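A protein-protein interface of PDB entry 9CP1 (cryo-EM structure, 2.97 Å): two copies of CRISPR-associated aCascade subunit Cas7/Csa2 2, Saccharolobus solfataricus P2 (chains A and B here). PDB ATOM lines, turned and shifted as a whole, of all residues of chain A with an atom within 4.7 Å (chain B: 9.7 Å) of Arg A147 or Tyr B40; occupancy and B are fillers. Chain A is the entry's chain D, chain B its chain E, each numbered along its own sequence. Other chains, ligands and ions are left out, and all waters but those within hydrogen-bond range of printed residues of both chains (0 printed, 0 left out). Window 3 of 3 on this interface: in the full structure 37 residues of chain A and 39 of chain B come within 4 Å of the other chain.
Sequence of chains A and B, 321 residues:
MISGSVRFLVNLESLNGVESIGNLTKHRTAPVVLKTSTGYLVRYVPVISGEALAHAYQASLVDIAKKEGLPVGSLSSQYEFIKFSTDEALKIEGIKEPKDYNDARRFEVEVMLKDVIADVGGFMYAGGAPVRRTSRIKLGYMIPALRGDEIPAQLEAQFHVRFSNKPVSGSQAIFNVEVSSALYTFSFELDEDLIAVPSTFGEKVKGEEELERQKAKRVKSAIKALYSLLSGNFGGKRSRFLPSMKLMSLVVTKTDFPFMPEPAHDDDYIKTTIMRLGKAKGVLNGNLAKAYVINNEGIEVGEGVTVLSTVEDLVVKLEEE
Of the 14 printed residues of chain B, 3 touch a printed residue of chain A. Along chain B the printed residues that touch a printed residue of chain A span positions 33 to 40. Printed residues of chain A that touch a printed residue of chain B: Arg A147, Pro A152, Met A248 and Glu A297. Among the printed residues, no Asp or Glu carboxylate lies within 4 Å of a Lys or Arg side-chain nitrogen of the other chain.
Ala A145 touches none of the printed residues of chain B. Arg A147 touches just one residue of chain B: Tyr B40 (3.1 Å). No residue of chain B comes within 4 Å of Gly A148. Of the printed residues of chain B, Met A248 touches Lys B35 and Tyr B40. Of the printed residues of chain B, Glu A297 touches Lys B35 and Tyr B40. Printed residues of chain A within 4 Å of Val B33: Pro A152 (3.5 Å). Printed residues of chain A within 4 Å of Lys B35: Met A248 (3.6 Å) and Glu A297 (3.7 Å). The nearest residue of chain B that does not touch Arg A147 is Gly B39 (5.3 Å). The nearest printed residue of chain A that does not touch Lys B35 is Arg A7 (7.3 Å).
Positions printed for both chains: 146 and 149. Of the 6 pairs that touch across the chains among the printed residues, none has its exchanged pair printed and touching as well.
NH2 of Arg A147 touches CD1 of Tyr B40, 3.1 Å away. Val B33 touches Pro A152. CD of Lys B35 touches CE of Met A248, at 3.6 Å. Met A248 touches Tyr B40. Glu A297 touches Lys B35 (CB to CE, 3.7 Å).
OH of Tyr B40 sits at hydrogen-bond distance from OE1 of Glu A297, 2.8 Å away.
The backbone carbonyl oxygen (O) of Arg A7 is in hydrogen-bond range of the backbone NH (N) of Met A248 (3.2 Å). The side-chain carboxylate (OE2) of Glu A297 is in salt-bridge range of the guanidinium group (NH1) of Arg A7, at 3.3 Å. NE of Arg A147 is in salt-bridge range of OD1 of Asp A267 (3.8 Å).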
ATOM      1  N   ARG A   7      12.340 -14.931  10.655  1.00  0.00           N
ATOM      2  CA  ARG A   7      13.134 -14.034  11.485  1.00  0.00           C
ATOM      3  C   ARG A   7      13.903 -13.058  10.602  1.00  0.00           C
ATOM      4  O   ARG A   7      14.567 -13.474   9.648  1.00  0.00           O
ATOM      5  CB  ARG A   7      14.093 -14.840  12.359  1.00  0.00           C
ATOM      6  CG  ARG A   7      15.010 -14.014  13.221  1.00  0.00           C
ATOM      7  CD  ARG A   7      15.931 -14.910  14.026  1.00  0.00           C
ATOM      8  NE  ARG A   7      15.299 -15.387  15.250  1.00  0.00           N
ATOM      9  CZ  ARG A   7      15.898 -16.155  16.149  1.00  0.00           C
ATOM     10  NH1 ARG A   7      17.142 -16.569  15.984  1.00  0.00           N
ATOM     11  NH2 ARG A   7      15.233 -16.510  17.243  1.00  0.00           N
ATOM     12  N   ALA A 145      12.677 -10.603  18.969  1.00  0.00           N
ATOM     13  CA  ALA A 145      12.797 -11.879  19.658  1.00  0.00           C
ATOM     14  C   ALA A 145      13.023 -11.674  21.151  1.00  0.00           C
ATOM     15  O   ALA A 145      13.921 -10.934  21.560  1.00  0.00           O
ATOM     16  CB  ALA A 145      13.944 -12.689  19.057  1.00  0.00           C
ATOM     17  N   LEU A 146      12.203 -12.341  21.963  1.00  0.00           N
ATOM     18  CA  LEU A 146      12.322 -12.278  23.420  1.00  0.00           C
ATOM     19  C   LEU A 146      13.230 -13.396  23.929  1.00  0.00           C
ATOM     20  O   LEU A 146      12.821 -14.297  24.658  1.00  0.00           O
ATOM     21  CB  LEU A 146      10.946 -12.352  24.068  1.00  0.00           C
ATOM     22  CG  LEU A 146       9.878 -11.388  23.563  1.00  0.00           C
ATOM     23  CD1 LEU A 146       8.563 -11.663  24.259  1.00  0.00           C
ATOM     24  CD2 LEU A 146      10.315  -9.961  23.801  1.00  0.00           C
ATOM     25  N   ARG A 147      14.490 -13.318  23.525  1.00  0.00           N
ATOM     26  CA  ARG A 147      15.487 -14.318  23.871  1.00  0.00           C
ATOM     27  C   ARG A 147      16.411 -13.779  24.953  1.00  0.00           C
ATOM     28  O   ARG A 147      16.794 -12.607  24.930  1.00  0.00           O
ATOM     29  CB  ARG A 147      16.307 -14.701  22.642  1.00  0.00           C
ATOM     30  CG  ARG A 147      17.312 -15.811  22.880  1.00  0.00           C
ATOM     31  CD  ARG A 147      18.026 -16.148  21.589  1.00  0.00           C
ATOM     32  NE  ARG A 147      18.077 -14.985  20.715  1.00  0.00           N
ATOM     33  CZ  ARG A 147      18.970 -14.012  20.820  1.00  0.00           C
ATOM     34  NH1 ARG A 147      19.936 -14.054  21.723  1.00  0.00           N
ATOM     35  NH2 ARG A 147      18.886 -12.965  20.006  1.00  0.00           N
ATOM     36  N   GLY A 148      16.771 -14.644  25.899  1.00  0.00           N
ATOM     37  CA  GLY A 148      17.716 -14.241  26.918  1.00  0.00           C
ATOM     38  C   GLY A 148      17.127 -13.237  27.899  1.00  0.00           C
ATOM     39  O   GLY A 148      15.917 -13.168  28.127  1.00  0.00           O
ATOM     40  N   ASP A 149      18.023 -12.443  28.485  1.00  0.00           N
ATOM     41  CA  ASP A 149      17.648 -11.450  29.481  1.00  0.00           C
ATOM     42  C   ASP A 149      17.618 -10.028  28.938  1.00  0.00           C
ATOM     43  O   ASP A 149      17.038  -9.150  29.584  1.00  0.00           O
ATOM     44  CB  ASP A 149      18.606 -11.512  30.675  1.00  0.00           C
ATOM     45  CG  ASP A 149      18.400 -12.749  31.521  1.00  0.00           C
ATOM     46  OD1 ASP A 149      17.635 -13.639  31.096  1.00  0.00           O
ATOM     47  OD2 ASP A 149      19.000 -12.831  32.613  1.00  0.00           O
ATOM     48  N   GLU A 150      18.223  -9.777  27.780  1.00  0.00           N
ATOM     49  CA  GLU A 150      18.275  -8.448  27.188  1.00  0.00           C
ATOM     50  C   GLU A 150      17.590  -8.473  25.831  1.00  0.00           C
ATOM     51  O   GLU A 150      17.920  -9.304  24.981  1.00  0.00           O
ATOM     52  CB  GLU A 150      19.720  -7.970  27.041  1.00  0.00           C
ATOM     53  CG  GLU A 150      20.568  -8.197  28.276  1.00  0.00           C
ATOM     54  CD  GLU A 150      21.954  -7.600  28.147  1.00  0.00           C
ATOM     55  OE1 GLU A 150      22.278  -7.076  27.061  1.00  0.00           O
ATOM     56  OE2 GLU A 150      22.720  -7.657  29.132  1.00  0.00           O
ATOM     57  N   PRO A 152      17.014  -7.484  22.170  1.00  0.00           N
ATOM     58  CA  PRO A 152      17.931  -6.955  21.140  1.00  0.00           C
ATOM     59  C   PRO A 152      17.276  -5.887  20.272  1.00  0.00           C
ATOM     60  O   PRO A 152      17.154  -6.007  19.050  1.00  0.00           O
ATOM     61  CB  PRO A 152      18.293  -8.216  20.354  1.00  0.00           C
ATOM     62  CG  PRO A 152      17.061  -9.056  20.437  1.00  0.00           C
ATOM     63  CD  PRO A 152      16.407  -8.763  21.764  1.00  0.00           C
ATOM     64  N   LEU A 183      15.629  -6.988  15.913  1.00  0.00           N
ATOM     65  CA  LEU A 183      15.647  -8.301  15.276  1.00  0.00           C
ATOM     66  C   LEU A 183      14.222  -8.841  15.365  1.00  0.00           C
ATOM     67  O   LEU A 183      13.842  -9.453  16.367  1.00  0.00           O
ATOM     68  CB  LEU A 183      16.664  -9.222  15.946  1.00  0.00           C
ATOM     69  CG  LEU A 183      16.642 -10.721  15.641  1.00  0.00           C
ATOM     70  CD1 LEU A 183      17.243 -11.007  14.281  1.00  0.00           C
ATOM     71  CD2 LEU A 183      17.395 -11.482  16.715  1.00  0.00           C
ATOM     72  N   MET A 248      17.254 -14.252   8.112  1.00  0.00           N
ATOM     73  CA  MET A 248      18.132 -15.044   8.966  1.00  0.00           C
ATOM     74  C   MET A 248      17.667 -16.476   9.168  1.00  0.00           C
ATOM     75  O   MET A 248      18.502 -17.380   9.235  1.00  0.00           O
ATOM     76  CB  MET A 248      18.288 -14.370  10.334  1.00  0.00           C
ATOM     77  CG  MET A 248      18.787 -12.940  10.270  1.00  0.00           C
ATOM     78  SD  MET A 248      20.473 -12.832   9.655  1.00  0.00           S
ATOM     79  CE  MET A 248      21.385 -13.083  11.171  1.00  0.00           C
ATOM     80  N   HIS A 265      11.348 -17.305  18.890  1.00  0.00           N
ATOM     81  CA  HIS A 265      11.899 -16.666  20.077  1.00  0.00           C
ATOM     82  C   HIS A 265      13.118 -17.380  20.631  1.00  0.00           C
ATOM     83  O   HIS A 265      14.068 -16.719  21.059  1.00  0.00           O
ATOM     84  CB  HIS A 265      10.833 -16.581  21.173  1.00  0.00           C
ATOM     85  CG  HIS A 265       9.756 -15.587  20.887  1.00  0.00           C
ATOM     86  ND1 HIS A 265       8.610 -15.491  21.645  1.00  0.00           N
ATOM     87  CD2 HIS A 265       9.654 -14.635  19.930  1.00  0.00           C
ATOM     88  CE1 HIS A 265       7.846 -14.528  21.164  1.00  0.00           C
ATOM     89  NE2 HIS A 265       8.455 -13.993  20.123  1.00  0.00           N
ATOM     90  N   ASP A 267      16.457 -20.005  20.369  1.00  0.00           N
ATOM     91  CA  ASP A 267      17.458 -20.359  19.368  1.00  0.00           C
ATOM     92  C   ASP A 267      17.187 -21.728  18.758  1.00  0.00           C
ATOM     93  O   ASP A 267      17.627 -22.003  17.636  1.00  0.00           O
ATOM     94  CB  ASP A 267      18.855 -20.323  19.985  1.00  0.00           C
ATOM     95  CG  ASP A 267      19.474 -18.941  19.945  1.00  0.00           C
ATOM     96  OD1 ASP A 267      19.191 -18.187  18.992  1.00  0.00           O
ATOM     97  OD2 ASP A 267      20.249 -18.610  20.867  1.00  0.00           O
ATOM     98  N   GLU A 297      22.247 -18.581   9.838  1.00  0.00           N
ATOM     99  CA  GLU A 297      22.937 -18.243  11.072  1.00  0.00           C
ATOM    100  C   GLU A 297      23.586 -19.441  11.748  1.00  0.00           C
ATOM    101  O   GLU A 297      24.142 -19.288  12.841  1.00  0.00           O
ATOM    102  CB  GLU A 297      21.972 -17.557  12.049  1.00  0.00           C
ATOM    103  CG  GLU A 297      20.619 -18.228  12.169  1.00  0.00           C
ATOM    104  CD  GLU A 297      19.691 -17.492  13.113  1.00  0.00           C
ATOM    105  OE1 GLU A 297      20.133 -16.499  13.725  1.00  0.00           O
ATOM    106  OE2 GLU A 297      18.519 -17.900  13.241  1.00  0.00           O
ATOM    107  N   VAL B  32      22.596   0.276  16.411  1.00  0.00           N
ATOM    108  CA  VAL B  32      22.548  -0.826  15.459  1.00  0.00           C
ATOM    109  C   VAL B  32      22.653  -2.144  16.213  1.00  0.00           C
ATOM    110  O   VAL B  32      23.378  -2.248  17.210  1.00  0.00           O
ATOM    111  CB  VAL B  32      23.663  -0.722  14.398  1.00  0.00           C
ATOM    112  CG1 VAL B  32      23.418   0.463  13.485  1.00  0.00           C
ATOM    113  CG2 VAL B  32      25.016  -0.603  15.066  1.00  0.00           C
ATOM    114  N   VAL B  33      21.918  -3.145  15.738  1.00  0.00           N
ATOM    115  CA  VAL B  33      21.941  -4.493  16.294  1.00  0.00           C
ATOM    116  C   VAL B  33      22.833  -5.348  15.406  1.00  0.00           C
ATOM    117  O   VAL B  33      22.614  -5.436  14.192  1.00  0.00           O
ATOM    118  CB  VAL B  33      20.528  -5.086  16.389  1.00  0.00           C
ATOM    119  CG1 VAL B  33      20.595  -6.551  16.760  1.00  0.00           C
ATOM    120  CG2 VAL B  33      19.696  -4.314  17.396  1.00  0.00           C
ATOM    121  N   LEU B  34      23.832  -5.985  16.008  1.00  0.00           N
ATOM    122  CA  LEU B  34      24.856  -6.708  15.272  1.00  0.00           C
ATOM    123  C   LEU B  34      24.934  -8.141  15.775  1.00  0.00           C
ATOM    124  O   LEU B  34      24.675  -8.409  16.951  1.00  0.00           O
ATOM    125  CB  LEU B  34      26.214  -6.016  15.421  1.00  0.00           C
ATOM    126  CG  LEU B  34      27.314  -6.355  14.419  1.00  0.00           C
ATOM    127  CD1 LEU B  34      28.180  -5.136  14.200  1.00  0.00           C
ATOM    128  CD2 LEU B  34      28.160  -7.509  14.903  1.00  0.00           C
ATOM    129  N   LYS B  35      25.284  -9.061  14.881  1.00  0.00           N
ATOM    130  CA  LYS B  35      25.422 -10.470  15.226  1.00  0.00           C
ATOM    131  C   LYS B  35      26.891 -10.862  15.290  1.00  0.00           C
ATOM    132  O   LYS B  35      27.633 -10.673  14.321  1.00  0.00           O
ATOM    133  CB  LYS B  35      24.698 -11.359  14.217  1.00  0.00           C
ATOM    134  CG  LYS B  35      24.794 -12.838  14.553  1.00  0.00           C
ATOM    135  CD  LYS B  35      24.027 -13.694  13.565  1.00  0.00           C
ATOM    136  CE  LYS B  35      24.009 -15.149  14.003  1.00  0.00           C
ATOM    137  NZ  LYS B  35      25.366 -15.758  13.955  1.00  0.00           N
ATOM    138  N   THR B  36      27.300 -11.419  16.425  1.00  0.00           N
ATOM    139  CA  THR B  36      28.629 -11.973  16.618  1.00  0.00           C
ATOM    140  C   THR B  36      28.511 -13.436  17.023  1.00  0.00           C
ATOM    141  O   THR B  36      27.417 -13.955  17.259  1.00  0.00           O
ATOM    142  CB  THR B  36      29.411 -11.200  17.686  1.00  0.00           C
ATOM    143  OG1 THR B  36      28.697 -11.243  18.927  1.00  0.00           O
ATOM    144  CG2 THR B  36      29.604  -9.757  17.269  1.00  0.00           C
ATOM    145  N   SER B  37      29.668 -14.095  17.122  1.00  0.00           N
ATOM    146  CA  SER B  37      29.699 -15.501  17.504  1.00  0.00           C
ATOM    147  C   SER B  37      29.090 -15.745  18.877  1.00  0.00           C
ATOM    148  O   SER B  37      28.660 -16.868  19.160  1.00  0.00           O
ATOM    149  CB  SER B  37      31.138 -16.018  17.474  1.00  0.00           C
ATOM    150  OG  SER B  37      31.891 -15.478  18.546  1.00  0.00           O
ATOM    151  N   THR B  38      29.039 -14.727  19.732  1.00  0.00           N
ATOM    152  CA  THR B  38      28.462 -14.858  21.061  1.00  0.00           C
ATOM    153  C   THR B  38      26.983 -14.494  21.110  1.00  0.00           C
ATOM    154  O   THR B  38      26.375 -14.588  22.181  1.00  0.00           O
ATOM    155  CB  THR B  38      29.229 -13.987  22.061  1.00  0.00           C
ATOM    156  OG1 THR B  38      29.295 -12.642  21.571  1.00  0.00           O
ATOM    157  CG2 THR B  38      30.640 -14.518  22.254  1.00  0.00           C
ATOM    158  N   GLY B  39      26.391 -14.081  19.992  1.00  0.00           N
ATOM    159  CA  GLY B  39      24.984 -13.736  19.993  1.00  0.00           C
ATOM    160  C   GLY B  39      24.670 -12.428  19.299  1.00  0.00           C
ATOM    161  O   GLY B  39      25.147 -12.177  18.190  1.00  0.00           O
ATOM    162  N   TYR B  40      23.864 -11.586  19.938  1.00  0.00           N
ATOM    163  CA  TYR B  40      23.436 -10.322  19.357  1.00  0.00           C
ATOM    164  C   TYR B  40      23.718  -9.186  20.327  1.00  0.00           C
ATOM    165  O   TYR B  40      23.469  -9.308  21.529  1.00  0.00           O
ATOM    166  CB  TYR B  40      21.949 -10.364  19.001  1.00  0.00           C
ATOM    167  CG  TYR B  40      21.630 -11.336  17.888  1.00  0.00           C
ATOM    168  CD1 TYR B  40      21.335 -12.661  18.163  1.00  0.00           C
ATOM    169  CD2 TYR B  40      21.627 -10.928  16.564  1.00  0.00           C
ATOM    170  CE1 TYR B  40      21.042 -13.551  17.154  1.00  0.00           C
ATOM    171  CE2 TYR B  40      21.337 -11.812  15.548  1.00  0.00           C
ATOM    172  CZ  TYR B  40      21.044 -13.122  15.849  1.00  0.00           C
ATOM    173  OH  TYR B  40      20.754 -14.009  14.841  1.00  0.00           O
ATOM    174  N   LEU B  41      24.228  -8.077  19.794  1.00  0.00           N
ATOM    175  CA  LEU B  41      24.662  -6.946  20.599  1.00  0.00           C
ATOM    176  C   LEU B  41      24.088  -5.654  20.036  1.00  0.00           C
ATOM    177  O   LEU B  41      23.682  -5.582  18.875  1.00  0.00           O
ATOM    178  CB  LEU B  41      26.191  -6.850  20.649  1.00  0.00           C
ATOM    179  CG  LEU B  41      26.922  -8.028  21.285  1.00  0.00           C
ATOM    180  CD1 LEU B  41      28.399  -7.975  20.947  1.00  0.00           C
ATOM    181  CD2 LEU B  41      26.717  -8.029  22.787  1.00  0.00           C
ATOM    182  N   VAL B  42      24.068  -4.626  20.883  1.00  0.00           N
ATOM    183  CA  VAL B  42      23.598  -3.293  20.522  1.00  0.00           C
ATOM    184  C   VAL B  42      24.777  -2.336  20.611  1.00  0.00           C
ATOM    185  O   VAL B  42      25.498  -2.327  21.615  1.00  0.00           O
ATOM    186  CB  VAL B  42      22.449  -2.831  21.437  1.00  0.00           C
ATOM    187  CG1 VAL B  42      21.876  -1.521  20.945  1.00  0.00           C
ATOM    188  CG2 VAL B  42      21.372  -3.895  21.502  1.00  0.00           C
ATOM    189  N   ARG B  43      24.976  -1.536  19.566  1.00  0.00           N
ATOM    190  CA  ARG B  43      26.105  -0.618  19.507  1.00  0.00           C
ATOM    191  C   ARG B  43      25.639   0.745  19.018  1.00  0.00           C
ATOM    192  O   ARG B  43      24.587   0.877  18.393  1.00  0.00           O
ATOM    193  CB  ARG B  43      27.210  -1.146  18.590  1.00  0.00           C
ATOM    194  CG  ARG B  43      27.924  -2.356  19.146  1.00  0.00           C
ATOM    195  CD  ARG B  43      29.073  -1.957  20.051  1.00  0.00           C
ATOM    196  NE  ARG B  43      29.489  -3.062  20.906  1.00  0.00           N
ATOM    197  CZ  ARG B  43      30.175  -4.117  20.491  1.00  0.00           C
ATOM    198  NH1 ARG B  43      30.568  -4.237  19.233  1.00  0.00           N
ATOM    199  NH2 ARG B  43      30.477  -5.077  21.361  1.00  0.00           N
ATOM    200  N   LEU B 146      28.101  -3.946   8.637  1.00  0.00           N
ATOM    201  CA  LEU B 146      28.081  -4.756   9.857  1.00  0.00           C
ATOM    202  C   LEU B 146      28.630  -6.156   9.580  1.00  0.00           C
ATOM    203  O   LEU B 146      27.940  -7.168   9.687  1.00  0.00           O
ATOM    204  CB  LEU B 146      26.670  -4.819  10.427  1.00  0.00           C
ATOM    205  CG  LEU B 146      25.941  -3.487  10.578  1.00  0.00           C
ATOM    206  CD1 LEU B 146      24.572  -3.701  11.191  1.00  0.00           C
ATOM    207  CD2 LEU B 146      26.759  -2.531  11.420  1.00  0.00           C
ATOM    208  N   ASP B 149      32.806  -9.350  13.678  1.00  0.00           N
ATOM    209  CA  ASP B 149      32.528  -9.009  15.066  1.00  0.00           C
ATOM    210  C   ASP B 149      32.974  -7.603  15.441  1.00  0.00           C
ATOM    211  O   ASP B 149      32.563  -7.103  16.495  1.00  0.00           O
ATOM    212  CB  ASP B 149      33.201 -10.018  16.005  1.00  0.00           C
ATOM    213  CG  ASP B 149      32.528 -11.375  15.981  1.00  0.00           C
ATOM    214  OD1 ASP B 149      31.656 -11.592  15.114  1.00  0.00           O
ATOM    215  OD2 ASP B 149      32.865 -12.224  16.834  1.00  0.00           O
